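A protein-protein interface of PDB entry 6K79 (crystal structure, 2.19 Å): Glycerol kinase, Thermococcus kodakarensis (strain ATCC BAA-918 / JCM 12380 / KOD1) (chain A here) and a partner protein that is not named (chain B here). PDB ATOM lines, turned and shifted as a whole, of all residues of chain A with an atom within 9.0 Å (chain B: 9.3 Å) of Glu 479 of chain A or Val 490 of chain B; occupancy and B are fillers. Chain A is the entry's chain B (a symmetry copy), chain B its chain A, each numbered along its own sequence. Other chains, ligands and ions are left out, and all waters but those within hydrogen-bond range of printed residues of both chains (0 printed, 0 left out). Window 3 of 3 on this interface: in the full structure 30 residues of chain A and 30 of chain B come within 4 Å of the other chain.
NH1 of Arg 483 of chain A lies within hydrogen-bond range of O of Arg 483 of chain B, 2.5 Å away. The guanidinium group of Arg 483 of chain B lies within hydrogen-bond range of the backbone carbonyl oxygen of Met 485 of chain A, at 2.7 Å. The guanidinium group of Arg 483 of chain A sits at hydrogen-bond distance from the backbone carbonyl oxygen of Met 485 of chain B (2.7 Å). The backbone carbonyl oxygen (O) of Gly 334 of chain A sits at hydrogen-bond distance from the indole nitrogen (NE1) of Trp 487 of chain B.
The backbone NH of Val 338 of chain A lies within hydrogen-bond range of the backbone carbonyl oxygen of Ile 356 of chain A (3.0 Å). N of Trp 487 of chain B is in hydrogen-bond range of O of Phe 352 of chain B (3.3 Å). The backbone carbonyl oxygen (O) of Tyr 336 of chain A lies within hydrogen-bond range of the backbone NH (N) of Ile 358 of chain A (3.0 Å). The side-chain hydroxyl of Tyr 336 of chain A is in hydrogen-bond range of the backbone carbonyl oxygen of Leu 473 of chain A (2.6 Å). N of Arg 354 of chain B sits at hydrogen-bond distance from O of Ala 484 of chain B (3.2 Å). OD1 of Asn 332 of chain A sits at hydrogen-bond distance from N of Gly 334 of chain A.
Among the printed residues, pairs that only touch across the chains: Ile 358 of chain A with Ile 356 of chain B, Ile 358 of chain A with Trp 487 of chain B, Glu 479 of chain A with Val 490 of chain B, Gly 476 of chain A with Trp 487 of chain B, Gly 334 of chain A with Val 491 of chain B, Arg 483 of chain A with Trp 487 of chain B, Ile 356 of chain A with Ile 356 of chain B, Glu 479 of chain A with Trp 487 of chain B, Arg 483 of chain A with Ala 484 of chain B, Ala 484 of chain A with Arg 483 of chain B, Ile 358 of chain A with Arg 483 of chain B, Ala 480 of chain A with Trp 487 of chain B and Tyr 336 of chain A with Trp 487 of chain B.
Printed residues of chain B within 4 Å of Gly 334 of chain A: Trp 487 (3.0 Å) and Val 491 (3.6 Å). Arg 472 of chain A touches none of the printed residues of chain B. Of the printed residues of chain B, Glu 479 of chain A touches Trp 487 (3.7 Å) and Val 490 (3.5 Å). Of chain B, only Trp 487 comes within 4 Å of Ala 480 of chain A. No residue of chain B comes within 4 Å of Lys 482 of chain A. Printed residues of chain B within 4 Å of Met 485 of chain A: Arg 483. Printed residues of chain A within 4 Å of Trp 487 of chain B: Gly 334 (3.0 Å), Tyr 336 (3.8 Å), Ile 358 (3.3 Å), Gly 476 (3.5 Å), Glu 479 (3.7 Å), Ala 480 (3.8 Å) and Arg 483 (3.7 Å). Lys 489 of chain B touches none of the printed residues of chain A. Val 490 of chain B touches just one residue of chain A: Glu 479 (3.5 Å). Of chain A, only Gly 334 (3.6 Å) comes within 4 Å of Val 491 of chain B. The nearest residue of chain B that does not touch Glu 479 of chain A is Val 491 of chain B (6.8 Å).
Along chain A the printed residues that touch a printed residue of chain B span positions 334 to 485. Of the 13 printed residues of chain B, 7 touch a printed residue of chain A. Printed residues of chain B that touch a printed residue of chain A: Ile 356, Arg 483, Ala 484, Met 485, Trp 487, Val 490 and Val 491. Hydrophobic or aromatic side chains of chain B within 4 Å of the printed part of chain A: Ile 356, Trp 487, Val 490 and Val 491. Among the printed residues, 17 pairs touch across the chains. Among the printed residues, no Asp or Glu carboxylate lies within 4 Å of a Lys or Arg side-chain nitrogen of the other chain.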
ATOM      1  N   ASN A 332      -1.841 -10.815   1.619  1.00  0.00           N
ATOM      2  CA  ASN A 332      -2.550 -11.758   0.750  1.00  0.00           C
ATOM      3  C   ASN A 332      -2.259 -11.450  -0.739  1.00  0.00           C
ATOM      4  O   ASN A 332      -2.687 -12.190  -1.628  1.00  0.00           O
ATOM      5  CB  ASN A 332      -4.047 -11.779   1.063  1.00  0.00           C
ATOM      6  CG  ASN A 332      -4.729 -10.440   0.843  1.00  0.00           C
ATOM      7  OD1 ASN A 332      -4.403  -9.729  -0.110  1.00  0.00           O
ATOM      8  ND2 ASN A 332      -5.674 -10.093   1.703  1.00  0.00           N
ATOM      9  N   GLY A 334      -3.700  -9.568  -2.726  1.00  0.00           N
ATOM     10  CA  GLY A 334      -4.942  -9.478  -3.504  1.00  0.00           C
ATOM     11  C   GLY A 334      -5.678 -10.810  -3.648  1.00  0.00           C
ATOM     12  O   GLY A 334      -6.745 -10.842  -4.241  1.00  0.00           O
ATOM     13  N   TYR A 336      -8.029 -13.750  -2.281  1.00  0.00           N
ATOM     14  CA  TYR A 336      -9.014 -14.104  -1.293  1.00  0.00           C
ATOM     15  C   TYR A 336      -9.693 -15.413  -1.680  1.00  0.00           C
ATOM     16  O   TYR A 336      -9.704 -15.794  -2.830  1.00  0.00           O
ATOM     17  CB  TYR A 336     -10.086 -13.020  -1.169  1.00  0.00           C
ATOM     18  CG  TYR A 336      -9.647 -11.761  -0.467  1.00  0.00           C
ATOM     19  CD1 TYR A 336      -8.722 -10.900  -1.039  1.00  0.00           C
ATOM     20  CD2 TYR A 336     -10.145 -11.430   0.777  1.00  0.00           C
ATOM     21  CE1 TYR A 336      -8.317  -9.728  -0.413  1.00  0.00           C
ATOM     22  CE2 TYR A 336      -9.740 -10.272   1.430  1.00  0.00           C
ATOM     23  CZ  TYR A 336      -8.836  -9.411   0.831  1.00  0.00           C
ATOM     24  OH  TYR A 336      -8.477  -8.252   1.470  1.00  0.00           O
ATOM     25  N   VAL A 338     -13.386 -17.242  -0.451  1.00  0.00           N
ATOM     26  CA  VAL A 338     -14.572 -17.350   0.311  1.00  0.00           C
ATOM     27  C   VAL A 338     -15.014 -18.809   0.228  1.00  0.00           C
ATOM     28  O   VAL A 338     -15.571 -19.161  -0.788  1.00  0.00           O
ATOM     29  CB  VAL A 338     -15.678 -16.436  -0.246  1.00  0.00           C
ATOM     30  CG1 VAL A 338     -16.955 -16.518   0.582  1.00  0.00           C
ATOM     31  CG2 VAL A 338     -15.204 -15.009  -0.391  1.00  0.00           C
ATOM     32  N   TYR A 348     -25.322 -12.332   5.155  1.00  0.00           N
ATOM     33  CA  TYR A 348     -25.702 -12.381   3.731  1.00  0.00           C
ATOM     34  C   TYR A 348     -26.850 -13.381   3.502  1.00  0.00           C
ATOM     35  O   TYR A 348     -27.724 -13.135   2.712  1.00  0.00           O
ATOM     36  CB  TYR A 348     -24.464 -12.728   2.903  1.00  0.00           C
ATOM     37  CG  TYR A 348     -23.173 -12.138   3.421  1.00  0.00           C
ATOM     38  CD1 TYR A 348     -22.817 -10.824   3.120  1.00  0.00           C
ATOM     39  CD2 TYR A 348     -22.309 -12.883   4.217  1.00  0.00           C
ATOM     40  CE1 TYR A 348     -21.632 -10.267   3.571  1.00  0.00           C
ATOM     41  CE2 TYR A 348     -21.114 -12.339   4.666  1.00  0.00           C
ATOM     42  CZ  TYR A 348     -20.775 -11.033   4.344  1.00  0.00           C
ATOM     43  OH  TYR A 348     -19.600 -10.491   4.795  1.00  0.00           O
ATOM     44  N   ILE A 356     -15.335 -19.405  -3.941  1.00  0.00           N
ATOM     45  CA  ILE A 356     -14.651 -18.611  -4.946  1.00  0.00           C
ATOM     46  C   ILE A 356     -13.226 -18.305  -4.478  1.00  0.00           C
ATOM     47  O   ILE A 356     -12.986 -17.971  -3.304  1.00  0.00           O
ATOM     48  CB  ILE A 356     -15.427 -17.316  -5.279  1.00  0.00           C
ATOM     49  CG1 ILE A 356     -14.645 -16.410  -6.232  1.00  0.00           C
ATOM     50  CG2 ILE A 356     -15.829 -16.559  -4.026  1.00  0.00           C
ATOM     51  CD1 ILE A 356     -15.343 -15.090  -6.508  1.00  0.00           C
ATOM     52  N   ILE A 358     -10.281 -15.660  -5.764  1.00  0.00           N
ATOM     53  CA  ILE A 358     -10.167 -14.534  -6.644  1.00  0.00           C
ATOM     54  C   ILE A 358      -8.840 -13.792  -6.414  1.00  0.00           C
ATOM     55  O   ILE A 358      -8.246 -13.811  -5.324  1.00  0.00           O
ATOM     56  CB  ILE A 358     -11.378 -13.604  -6.466  1.00  0.00           C
ATOM     57  CG1 ILE A 358     -11.436 -12.566  -7.584  1.00  0.00           C
ATOM     58  CG2 ILE A 358     -11.394 -12.956  -5.081  1.00  0.00           C
ATOM     59  CD1 ILE A 358     -12.684 -11.762  -7.562  1.00  0.00           C
ATOM     60  N   GLU A 471      -9.374  -2.116   7.463  1.00  0.00           N
ATOM     61  CA  GLU A 471     -10.537  -1.735   6.639  1.00  0.00           C
ATOM     62  C   GLU A 471     -10.245  -2.059   5.162  1.00  0.00           C
ATOM     63  O   GLU A 471     -11.120  -2.536   4.471  1.00  0.00           O
ATOM     64  CB  GLU A 471     -10.946  -0.281   6.903  1.00  0.00           C
ATOM     65  CG  GLU A 471     -11.775  -0.113   8.178  1.00  0.00           C
ATOM     66  CD  GLU A 471     -12.665  -1.297   8.570  1.00  0.00           C
ATOM     67  OE1 GLU A 471     -13.772  -1.435   7.930  1.00  0.00           O
ATOM     68  OE2 GLU A 471     -12.261  -2.109   9.517  1.00  0.00           O
ATOM     69  N   ARG A 472      -9.027  -1.904   4.691  1.00  0.00           N
ATOM     70  CA  ARG A 472      -8.751  -2.311   3.306  1.00  0.00           C
ATOM     71  C   ARG A 472      -8.860  -3.855   3.192  1.00  0.00           C
ATOM     72  O   ARG A 472      -9.429  -4.344   2.232  1.00  0.00           O
ATOM     73  CB  ARG A 472      -7.406  -1.746   2.843  1.00  0.00           C
ATOM     74  CG  ARG A 472      -6.989  -2.210   1.453  1.00  0.00           C
ATOM     75  CD  ARG A 472      -5.561  -1.827   1.074  1.00  0.00           C
ATOM     76  NE  ARG A 472      -4.585  -1.985   2.156  1.00  0.00           N
ATOM     77  CZ  ARG A 472      -3.689  -2.971   2.255  1.00  0.00           C
ATOM     78  NH1 ARG A 472      -3.656  -3.949   1.366  1.00  0.00           N
ATOM     79  NH2 ARG A 472      -2.829  -2.984   3.255  1.00  0.00           N
ATOM     80  N   LEU A 473      -8.376  -4.629   4.181  1.00  0.00           N
ATOM     81  CA  LEU A 473      -8.368  -6.084   4.017  1.00  0.00           C
ATOM     82  C   LEU A 473      -9.806  -6.592   4.065  1.00  0.00           C
ATOM     83  O   LEU A 473     -10.216  -7.438   3.251  1.00  0.00           O
ATOM     84  CB  LEU A 473      -7.510  -6.733   5.110  1.00  0.00           C
ATOM     85  CG  LEU A 473      -5.998  -6.531   4.970  1.00  0.00           C
ATOM     86  CD1 LEU A 473      -5.258  -7.240   6.079  1.00  0.00           C
ATOM     87  CD2 LEU A 473      -5.505  -6.975   3.606  1.00  0.00           C
ATOM     88  N   TYR A 474     -10.562  -6.073   5.016  1.00  0.00           N
ATOM     89  CA  TYR A 474     -11.940  -6.484   5.208  1.00  0.00           C
ATOM     90  C   TYR A 474     -12.779  -6.088   3.987  1.00  0.00           C
ATOM     91  O   TYR A 474     -13.696  -6.789   3.647  1.00  0.00           O
ATOM     92  CB  TYR A 474     -12.538  -5.890   6.487  1.00  0.00           C
ATOM     93  CG  TYR A 474     -13.781  -6.580   6.981  1.00  0.00           C
ATOM     94  CD1 TYR A 474     -13.839  -7.968   7.020  1.00  0.00           C
ATOM     95  CD2 TYR A 474     -14.875  -5.875   7.467  1.00  0.00           C
ATOM     96  CE1 TYR A 474     -14.957  -8.635   7.490  1.00  0.00           C
ATOM     97  CE2 TYR A 474     -16.022  -6.528   7.911  1.00  0.00           C
ATOM     98  CZ  TYR A 474     -16.047  -7.913   7.930  1.00  0.00           C
ATOM     99  OH  TYR A 474     -17.107  -8.642   8.357  1.00  0.00           O
ATOM    100  N   LYS A 475     -12.480  -4.955   3.369  1.00  0.00           N
ATOM    101  CA  LYS A 475     -13.181  -4.494   2.177  1.00  0.00           C
ATOM    102  C   LYS A 475     -12.993  -5.526   1.052  1.00  0.00           C
ATOM    103  O   LYS A 475     -13.946  -5.864   0.340  1.00  0.00           O
ATOM    104  CB  LYS A 475     -12.639  -3.124   1.743  1.00  0.00           C
ATOM    105  CG  LYS A 475     -13.459  -2.403   0.677  1.00  0.00           C
ATOM    106  CD  LYS A 475     -12.676  -1.348  -0.117  1.00  0.00           C
ATOM    107  CE  LYS A 475     -13.424  -0.036  -0.304  1.00  0.00           C
ATOM    108  NZ  LYS A 475     -14.617  -0.171  -1.181  1.00  0.00           N
ATOM    109  N   GLY A 476     -11.750  -5.977   0.881  1.00  0.00           N
ATOM    110  CA  GLY A 476     -11.466  -7.048  -0.049  1.00  0.00           C
ATOM    111  C   GLY A 476     -12.367  -8.243   0.208  1.00  0.00           C
ATOM    112  O   GLY A 476     -12.951  -8.837  -0.722  1.00  0.00           O
ATOM    113  N   TRP A 477     -12.526  -8.595   1.477  1.00  0.00           N
ATOM    114  CA  TRP A 477     -13.285  -9.789   1.833  1.00  0.00           C
ATOM    115  C   TRP A 477     -14.738  -9.643   1.391  1.00  0.00           C
ATOM    116  O   TRP A 477     -15.305 -10.569   0.780  1.00  0.00           O
ATOM    117  CB  TRP A 477     -13.210 -10.077   3.340  1.00  0.00           C
ATOM    118  CG  TRP A 477     -14.218 -11.072   3.821  1.00  0.00           C
ATOM    119  CD1 TRP A 477     -15.344 -10.822   4.546  1.00  0.00           C
ATOM    120  CD2 TRP A 477     -14.214 -12.483   3.583  1.00  0.00           C
ATOM    121  NE1 TRP A 477     -16.017 -11.992   4.812  1.00  0.00           N
ATOM    122  CE2 TRP A 477     -15.332 -13.027   4.249  1.00  0.00           C
ATOM    123  CE3 TRP A 477     -13.328 -13.346   2.949  1.00  0.00           C
ATOM    124  CZ2 TRP A 477     -15.620 -14.386   4.246  1.00  0.00           C
ATOM    125  CZ3 TRP A 477     -13.611 -14.697   2.951  1.00  0.00           C
ATOM    126  CH2 TRP A 477     -14.737 -15.202   3.594  1.00  0.00           C
ATOM    127  N   LYS A 478     -15.327  -8.495   1.737  1.00  0.00           N
ATOM    128  CA  LYS A 478     -16.752  -8.209   1.398  1.00  0.00           C
ATOM    129  C   LYS A 478     -16.942  -8.186  -0.120  1.00  0.00           C
ATOM    130  O   LYS A 478     -17.953  -8.672  -0.603  1.00  0.00           O
ATOM    131  CB  LYS A 478     -17.243  -6.900   2.029  1.00  0.00           C
ATOM    132  CG  LYS A 478     -17.671  -7.061   3.487  1.00  0.00           C
ATOM    133  CD  LYS A 478     -18.035  -5.771   4.227  1.00  0.00           C
ATOM    134  CE  LYS A 478     -17.068  -4.626   3.985  1.00  0.00           C
ATOM    135  NZ  LYS A 478     -17.176  -3.572   5.030  1.00  0.00           N
ATOM    136  N   GLU A 479     -15.982  -7.653  -0.851  1.00  0.00           N
ATOM    137  CA  GLU A 479     -16.075  -7.669  -2.315  1.00  0.00           C
ATOM    138  C   GLU A 479     -16.051  -9.112  -2.863  1.00  0.00           C
ATOM    139  O   GLU A 479     -16.805  -9.440  -3.806  1.00  0.00           O
ATOM    140  CB  GLU A 479     -14.948  -6.832  -2.918  1.00  0.00           C
ATOM    141  CG  GLU A 479     -15.118  -5.345  -2.651  1.00  0.00           C
ATOM    142  CD  GLU A 479     -16.041  -4.593  -3.600  1.00  0.00           C
ATOM    143  OE1 GLU A 479     -16.745  -5.261  -4.410  1.00  0.00           O
ATOM    144  OE2 GLU A 479     -16.042  -3.328  -3.532  1.00  0.00           O
ATOM    145  N   ALA A 480     -15.217  -9.974  -2.276  1.00  0.00           N
ATOM    146  CA  ALA A 480     -15.109 -11.377  -2.725  1.00  0.00           C
ATOM    147  C   ALA A 480     -16.399 -12.105  -2.385  1.00  0.00           C
ATOM    148  O   ALA A 480     -16.909 -12.880  -3.192  1.00  0.00           O
ATOM    149  CB  ALA A 480     -13.909 -12.057  -2.116  1.00  0.00           C
ATOM    150  N   VAL A 481     -16.951 -11.799  -1.219  1.00  0.00           N
ATOM    151  CA  VAL A 481     -18.184 -12.434  -0.784  1.00  0.00           C
ATOM    152  C   VAL A 481     -19.286 -12.115  -1.805  1.00  0.00           C
ATOM    153  O   VAL A 481     -20.050 -13.021  -2.169  1.00  0.00           O
ATOM    154  CB  VAL A 481     -18.601 -12.005   0.641  1.00  0.00           C
ATOM    155  CG1 VAL A 481     -20.065 -12.312   0.902  1.00  0.00           C
ATOM    156  CG2 VAL A 481     -17.719 -12.635   1.712  1.00  0.00           C
ATOM    157  N   LYS A 482     -19.367 -10.860  -2.253  1.00  0.00           N
ATOM    158  CA  LYS A 482     -20.397 -10.447  -3.239  1.00  0.00           C
ATOM    159  C   LYS A 482     -20.258 -11.235  -4.556  1.00  0.00           C
ATOM    160  O   LYS A 482     -21.254 -11.491  -5.207  1.00  0.00           O
ATOM    161  CB  LYS A 482     -20.315  -8.946  -3.564  1.00  0.00           C
ATOM    162  CG  LYS A 482     -20.653  -8.008  -2.409  1.00  0.00           C
ATOM    163  CD  LYS A 482     -20.218  -6.571  -2.652  1.00  0.00           C
ATOM    164  CE  LYS A 482     -20.443  -5.659  -1.462  1.00  0.00           C
ATOM    165  NZ  LYS A 482     -19.390  -4.620  -1.379  1.00  0.00           N
ATOM    166  N   ARG A 483     -19.037 -11.593  -4.940  1.00  0.00           N
ATOM    167  CA  ARG A 483     -18.817 -12.310  -6.176  1.00  0.00           C
ATOM    168  C   ARG A 483     -19.155 -13.798  -6.025  1.00  0.00           C
ATOM    169  O   ARG A 483     -19.240 -14.493  -7.051  1.00  0.00           O
ATOM    170  CB  ARG A 483     -17.386 -12.080  -6.661  1.00  0.00           C
ATOM    171  CG  ARG A 483     -17.208 -10.673  -7.208  1.00  0.00           C
ATOM    172  CD  ARG A 483     -15.795 -10.189  -7.186  1.00  0.00           C
ATOM    173  NE  ARG A 483     -15.793  -8.743  -7.394  1.00  0.00           N
ATOM    174  CZ  ARG A 483     -15.244  -8.132  -8.431  1.00  0.00           C
ATOM    175  NH1 ARG A 483     -14.758  -8.845  -9.441  1.00  0.00           N
ATOM    176  NH2 ARG A 483     -15.152  -6.813  -8.443  1.00  0.00           N
ATOM    177  N   ALA A 484     -19.337 -14.281  -4.793  1.00  0.00           N
ATOM    178  CA  ALA A 484     -19.695 -15.695  -4.545  1.00  0.00           C
ATOM    179  C   ALA A 484     -21.224 -15.898  -4.590  1.00  0.00           C
ATOM    180  O   ALA A 484     -21.715 -17.019  -4.778  1.00  0.00           O
ATOM    181  CB  ALA A 484     -19.121 -16.132  -3.225  1.00  0.00           C
ATOM    182  N   MET A 485     -21.984 -14.816  -4.459  1.00  0.00           N
ATOM    183  CA  MET A 485     -23.425 -14.896  -4.238  1.00  0.00           C
ATOM    184  C   MET A 485     -24.170 -15.383  -5.499  1.00  0.00           C
ATOM    185  O   MET A 485     -23.796 -15.052  -6.635  1.00  0.00           O
ATOM    186  CB  MET A 485     -23.954 -13.522  -3.801  1.00  0.00           C
ATOM    187  CG  MET A 485     -23.444 -13.115  -2.430  1.00  0.00           C
ATOM    188  SD  MET A 485     -24.300 -11.686  -1.714  1.00  0.00           S
ATOM    189  CE  MET A 485     -23.659 -10.361  -2.718  1.00  0.00           C
ATOM    190  N   PHE B 352      -8.294  -4.575 -15.277  1.00  0.00           N
ATOM    191  CA  PHE B 352      -8.260  -4.773 -13.818  1.00  0.00           C
ATOM    192  C   PHE B 352      -8.812  -6.155 -13.402  1.00  0.00           C
ATOM    193  O   PHE B 352      -8.666  -6.540 -12.227  1.00  0.00           O
ATOM    194  CB  PHE B 352      -8.950  -3.587 -13.147  1.00  0.00           C
ATOM    195  CG  PHE B 352      -8.266  -2.290 -13.493  1.00  0.00           C
ATOM    196  CD1 PHE B 352      -6.976  -2.045 -13.048  1.00  0.00           C
ATOM    197  CD2 PHE B 352      -8.884  -1.354 -14.312  1.00  0.00           C
ATOM    198  CE1 PHE B 352      -6.324  -0.866 -13.388  1.00  0.00           C
ATOM    199  CE2 PHE B 352      -8.236  -0.175 -14.653  1.00  0.00           C
ATOM    200  CZ  PHE B 352      -6.953   0.062 -14.194  1.00  0.00           C
ATOM    201  N   ALA B 353      -9.388  -6.928 -14.342  1.00  0.00           N
ATOM    202  CA  ALA B 353      -9.859  -8.262 -14.025  1.00  0.00           C
ATOM    203  C   ALA B 353      -8.669  -9.108 -13.550  1.00  0.00           C
ATOM    204  O   ALA B 353      -7.510  -8.880 -13.922  1.00  0.00           O
ATOM    205  CB  ALA B 353     -10.546  -8.887 -15.230  1.00  0.00           C
ATOM    206  N   ARG B 354      -8.949 -10.052 -12.676  1.00  0.00           N
ATOM    207  CA  ARG B 354      -7.931 -11.007 -12.276  1.00  0.00           C
ATOM    208  C   ARG B 354      -8.584 -12.383 -12.279  1.00  0.00           C
ATOM    209  O   ARG B 354      -9.796 -12.490 -12.423  1.00  0.00           O
ATOM    210  CB  ARG B 354      -7.378 -10.657 -10.895  1.00  0.00           C
ATOM    211  CG  ARG B 354      -6.606  -9.350 -10.820  1.00  0.00           C
ATOM    212  CD  ARG B 354      -5.290  -9.443 -11.549  1.00  0.00           C
ATOM    213  NE  ARG B 354      -4.590  -8.170 -11.527  1.00  0.00           N
ATOM    214  CZ  ARG B 354      -4.653  -7.239 -12.479  1.00  0.00           C
ATOM    215  NH1 ARG B 354      -5.455  -7.377 -13.521  1.00  0.00           N
ATOM    216  NH2 ARG B 354      -3.893  -6.166 -12.378  1.00  0.00           N
ATOM    217  N   ILE B 356     -10.194 -15.940 -11.324  1.00  0.00           N
ATOM    218  CA  ILE B 356     -11.281 -16.433 -10.462  1.00  0.00           C
ATOM    219  C   ILE B 356     -11.438 -17.933 -10.721  1.00  0.00           C
ATOM    220  O   ILE B 356     -11.512 -18.396 -11.886  1.00  0.00           O
ATOM    221  CB  ILE B 356     -12.626 -15.713 -10.750  1.00  0.00           C
ATOM    222  CG1 ILE B 356     -12.485 -14.204 -10.630  1.00  0.00           C
ATOM    223  CG2 ILE B 356     -13.751 -16.179  -9.840  1.00  0.00           C
ATOM    224  CD1 ILE B 356     -13.619 -13.553  -9.846  1.00  0.00           C
ATOM    225  N   ARG B 483     -17.756 -11.786 -12.804  1.00  0.00           N
ATOM    226  CA  ARG B 483     -17.263 -11.780 -11.409  1.00  0.00           C
ATOM    227  C   ARG B 483     -15.738 -11.572 -11.332  1.00  0.00           C
ATOM    228  O   ARG B 483     -15.256 -11.192 -10.294  1.00  0.00           O
ATOM    229  CB  ARG B 483     -17.762 -13.052 -10.721  1.00  0.00           C
ATOM    230  CG  ARG B 483     -19.272 -13.029 -10.566  1.00  0.00           C
ATOM    231  CD  ARG B 483     -19.823 -14.402 -10.322  1.00  0.00           C
ATOM    232  NE  ARG B 483     -21.276 -14.387 -10.409  1.00  0.00           N
ATOM    233  CZ  ARG B 483     -22.085 -14.720  -9.435  1.00  0.00           C
ATOM    234  NH1 ARG B 483     -21.602 -14.998  -8.230  1.00  0.00           N
ATOM    235  NH2 ARG B 483     -23.381 -14.739  -9.659  1.00  0.00           N
ATOM    236  N   ALA B 484     -14.992 -11.783 -12.416  1.00  0.00           N
ATOM    237  CA  ALA B 484     -13.539 -11.541 -12.463  1.00  0.00           C
ATOM    238  C   ALA B 484     -13.243 -10.050 -12.630  1.00  0.00           C
ATOM    239  O   ALA B 484     -12.112  -9.594 -12.333  1.00  0.00           O
ATOM    240  CB  ALA B 484     -12.916 -12.326 -13.595  1.00  0.00           C
ATOM    241  N   MET B 485     -14.238  -9.306 -13.104  1.00  0.00           N
ATOM    242  CA  MET B 485     -14.010  -7.930 -13.617  1.00  0.00           C
ATOM    243  C   MET B 485     -13.785  -6.944 -12.457  1.00  0.00           C
ATOM    244  O   MET B 485     -14.423  -7.056 -11.396  1.00  0.00           O
ATOM    245  CB  MET B 485     -15.205  -7.431 -14.439  1.00  0.00           C
ATOM    246  CG  MET B 485     -15.269  -7.981 -15.847  1.00  0.00           C
ATOM    247  SD  MET B 485     -16.874  -7.592 -16.593  1.00  0.00           S
ATOM    248  CE  MET B 485     -16.617  -8.221 -18.247  1.00  0.00           C
ATOM    249  N   GLY B 486     -12.880  -5.992 -12.685  1.00  0.00           N
ATOM    250  CA  GLY B 486     -12.680  -4.908 -11.780  1.00  0.00           C
ATOM    251  C   GLY B 486     -11.946  -5.289 -10.495  1.00  0.00           C
ATOM    252  O   GLY B 486     -11.815  -4.450  -9.620  1.00  0.00           O
ATOM    253  N   TRP B 487     -11.421  -6.515 -10.358  1.00  0.00           N
ATOM    254  CA  TRP B 487     -10.899  -6.947  -9.068  1.00  0.00           C
ATOM    255  C   TRP B 487      -9.682  -6.100  -8.660  1.00  0.00           C
ATOM    256  O   TRP B 487      -9.567  -5.754  -7.499  1.00  0.00           O
ATOM    257  CB  TRP B 487     -10.563  -8.441  -9.071  1.00  0.00           C
ATOM    258  CG  TRP B 487     -10.093  -8.917  -7.728  1.00  0.00           C
ATOM    259  CD1 TRP B 487      -8.820  -9.257  -7.361  1.00  0.00           C
ATOM    260  CD2 TRP B 487     -10.895  -9.018  -6.549  1.00  0.00           C
ATOM    261  NE1 TRP B 487      -8.786  -9.625  -6.051  1.00  0.00           N
ATOM    262  CE2 TRP B 487     -10.036  -9.457  -5.514  1.00  0.00           C
ATOM    263  CE3 TRP B 487     -12.243  -8.773  -6.270  1.00  0.00           C
ATOM    264  CZ2 TRP B 487     -10.497  -9.661  -4.216  1.00  0.00           C
ATOM    265  CZ3 TRP B 487     -12.697  -8.968  -4.987  1.00  0.00           C
ATOM    266  CH2 TRP B 487     -11.836  -9.419  -3.983  1.00  0.00           C
ATOM    267  N   ALA B 488      -8.800  -5.715  -9.578  1.00  0.00           N
ATOM    268  CA  ALA B 488      -7.625  -4.986  -9.136  1.00  0.00           C
ATOM    269  C   ALA B 488      -7.968  -3.525  -8.794  1.00  0.00           C
ATOM    270  O   ALA B 488      -7.108  -2.841  -8.325  1.00  0.00           O
ATOM    271  CB  ALA B 488      -6.530  -5.058 -10.163  1.00  0.00           C
ATOM    272  N   LYS B 489      -9.194  -3.052  -9.026  1.00  0.00           N
ATOM    273  CA  LYS B 489      -9.658  -1.787  -8.438  1.00  0.00           C
ATOM    274  C   LYS B 489     -10.090  -1.969  -6.970  1.00  0.00           C
ATOM    275  O   LYS B 489     -10.287  -0.990  -6.300  1.00  0.00           O
ATOM    276  CB  LYS B 489     -10.821  -1.203  -9.247  1.00  0.00           C
ATOM    277  CG  LYS B 489     -10.543  -1.086 -10.740  1.00  0.00           C
ATOM    278  CD  LYS B 489     -11.468  -0.150 -11.495  1.00  0.00           C
ATOM    279  CE  LYS B 489     -12.910  -0.205 -11.046  1.00  0.00           C
ATOM    280  NZ  LYS B 489     -13.834   0.129 -12.156  1.00  0.00           N
ATOM    281  N   VAL B 490     -10.219  -3.197  -6.461  1.00  0.00           N
ATOM    282  CA  VAL B 490     -10.660  -3.490  -5.075  1.00  0.00           C
ATOM    283  C   VAL B 490      -9.451  -3.691  -4.153  1.00  0.00           C
ATOM    284  O   VAL B 490      -9.524  -3.343  -2.991  1.00  0.00           O
ATOM    285  CB  VAL B 490     -11.567  -4.735  -5.046  1.00  0.00           C
ATOM    286  CG1 VAL B 490     -11.808  -5.223  -3.623  1.00  0.00           C
ATOM    287  CG2 VAL B 490     -12.885  -4.484  -5.768  1.00  0.00           C
ATOM    288  N   VAL B 491      -8.343  -4.213  -4.658  1.00  0.00           N
ATOM    289  CA  VAL B 491      -7.167  -4.519  -3.837  1.00  0.00           C
ATOM    290  C   VAL B 491      -5.934  -3.810  -4.409  1.00  0.00           C
ATOM    291  O   VAL B 491      -4.902  -3.699  -3.710  1.00  0.00           O
ATOM    292  CB  VAL B 491      -6.941  -6.046  -3.752  1.00  0.00           C
ATOM    293  CG1 VAL B 491      -8.205  -6.780  -3.316  1.00  0.00           C
ATOM    294  CG2 VAL B 491      -6.413  -6.637  -5.060  1.00  0.00           C
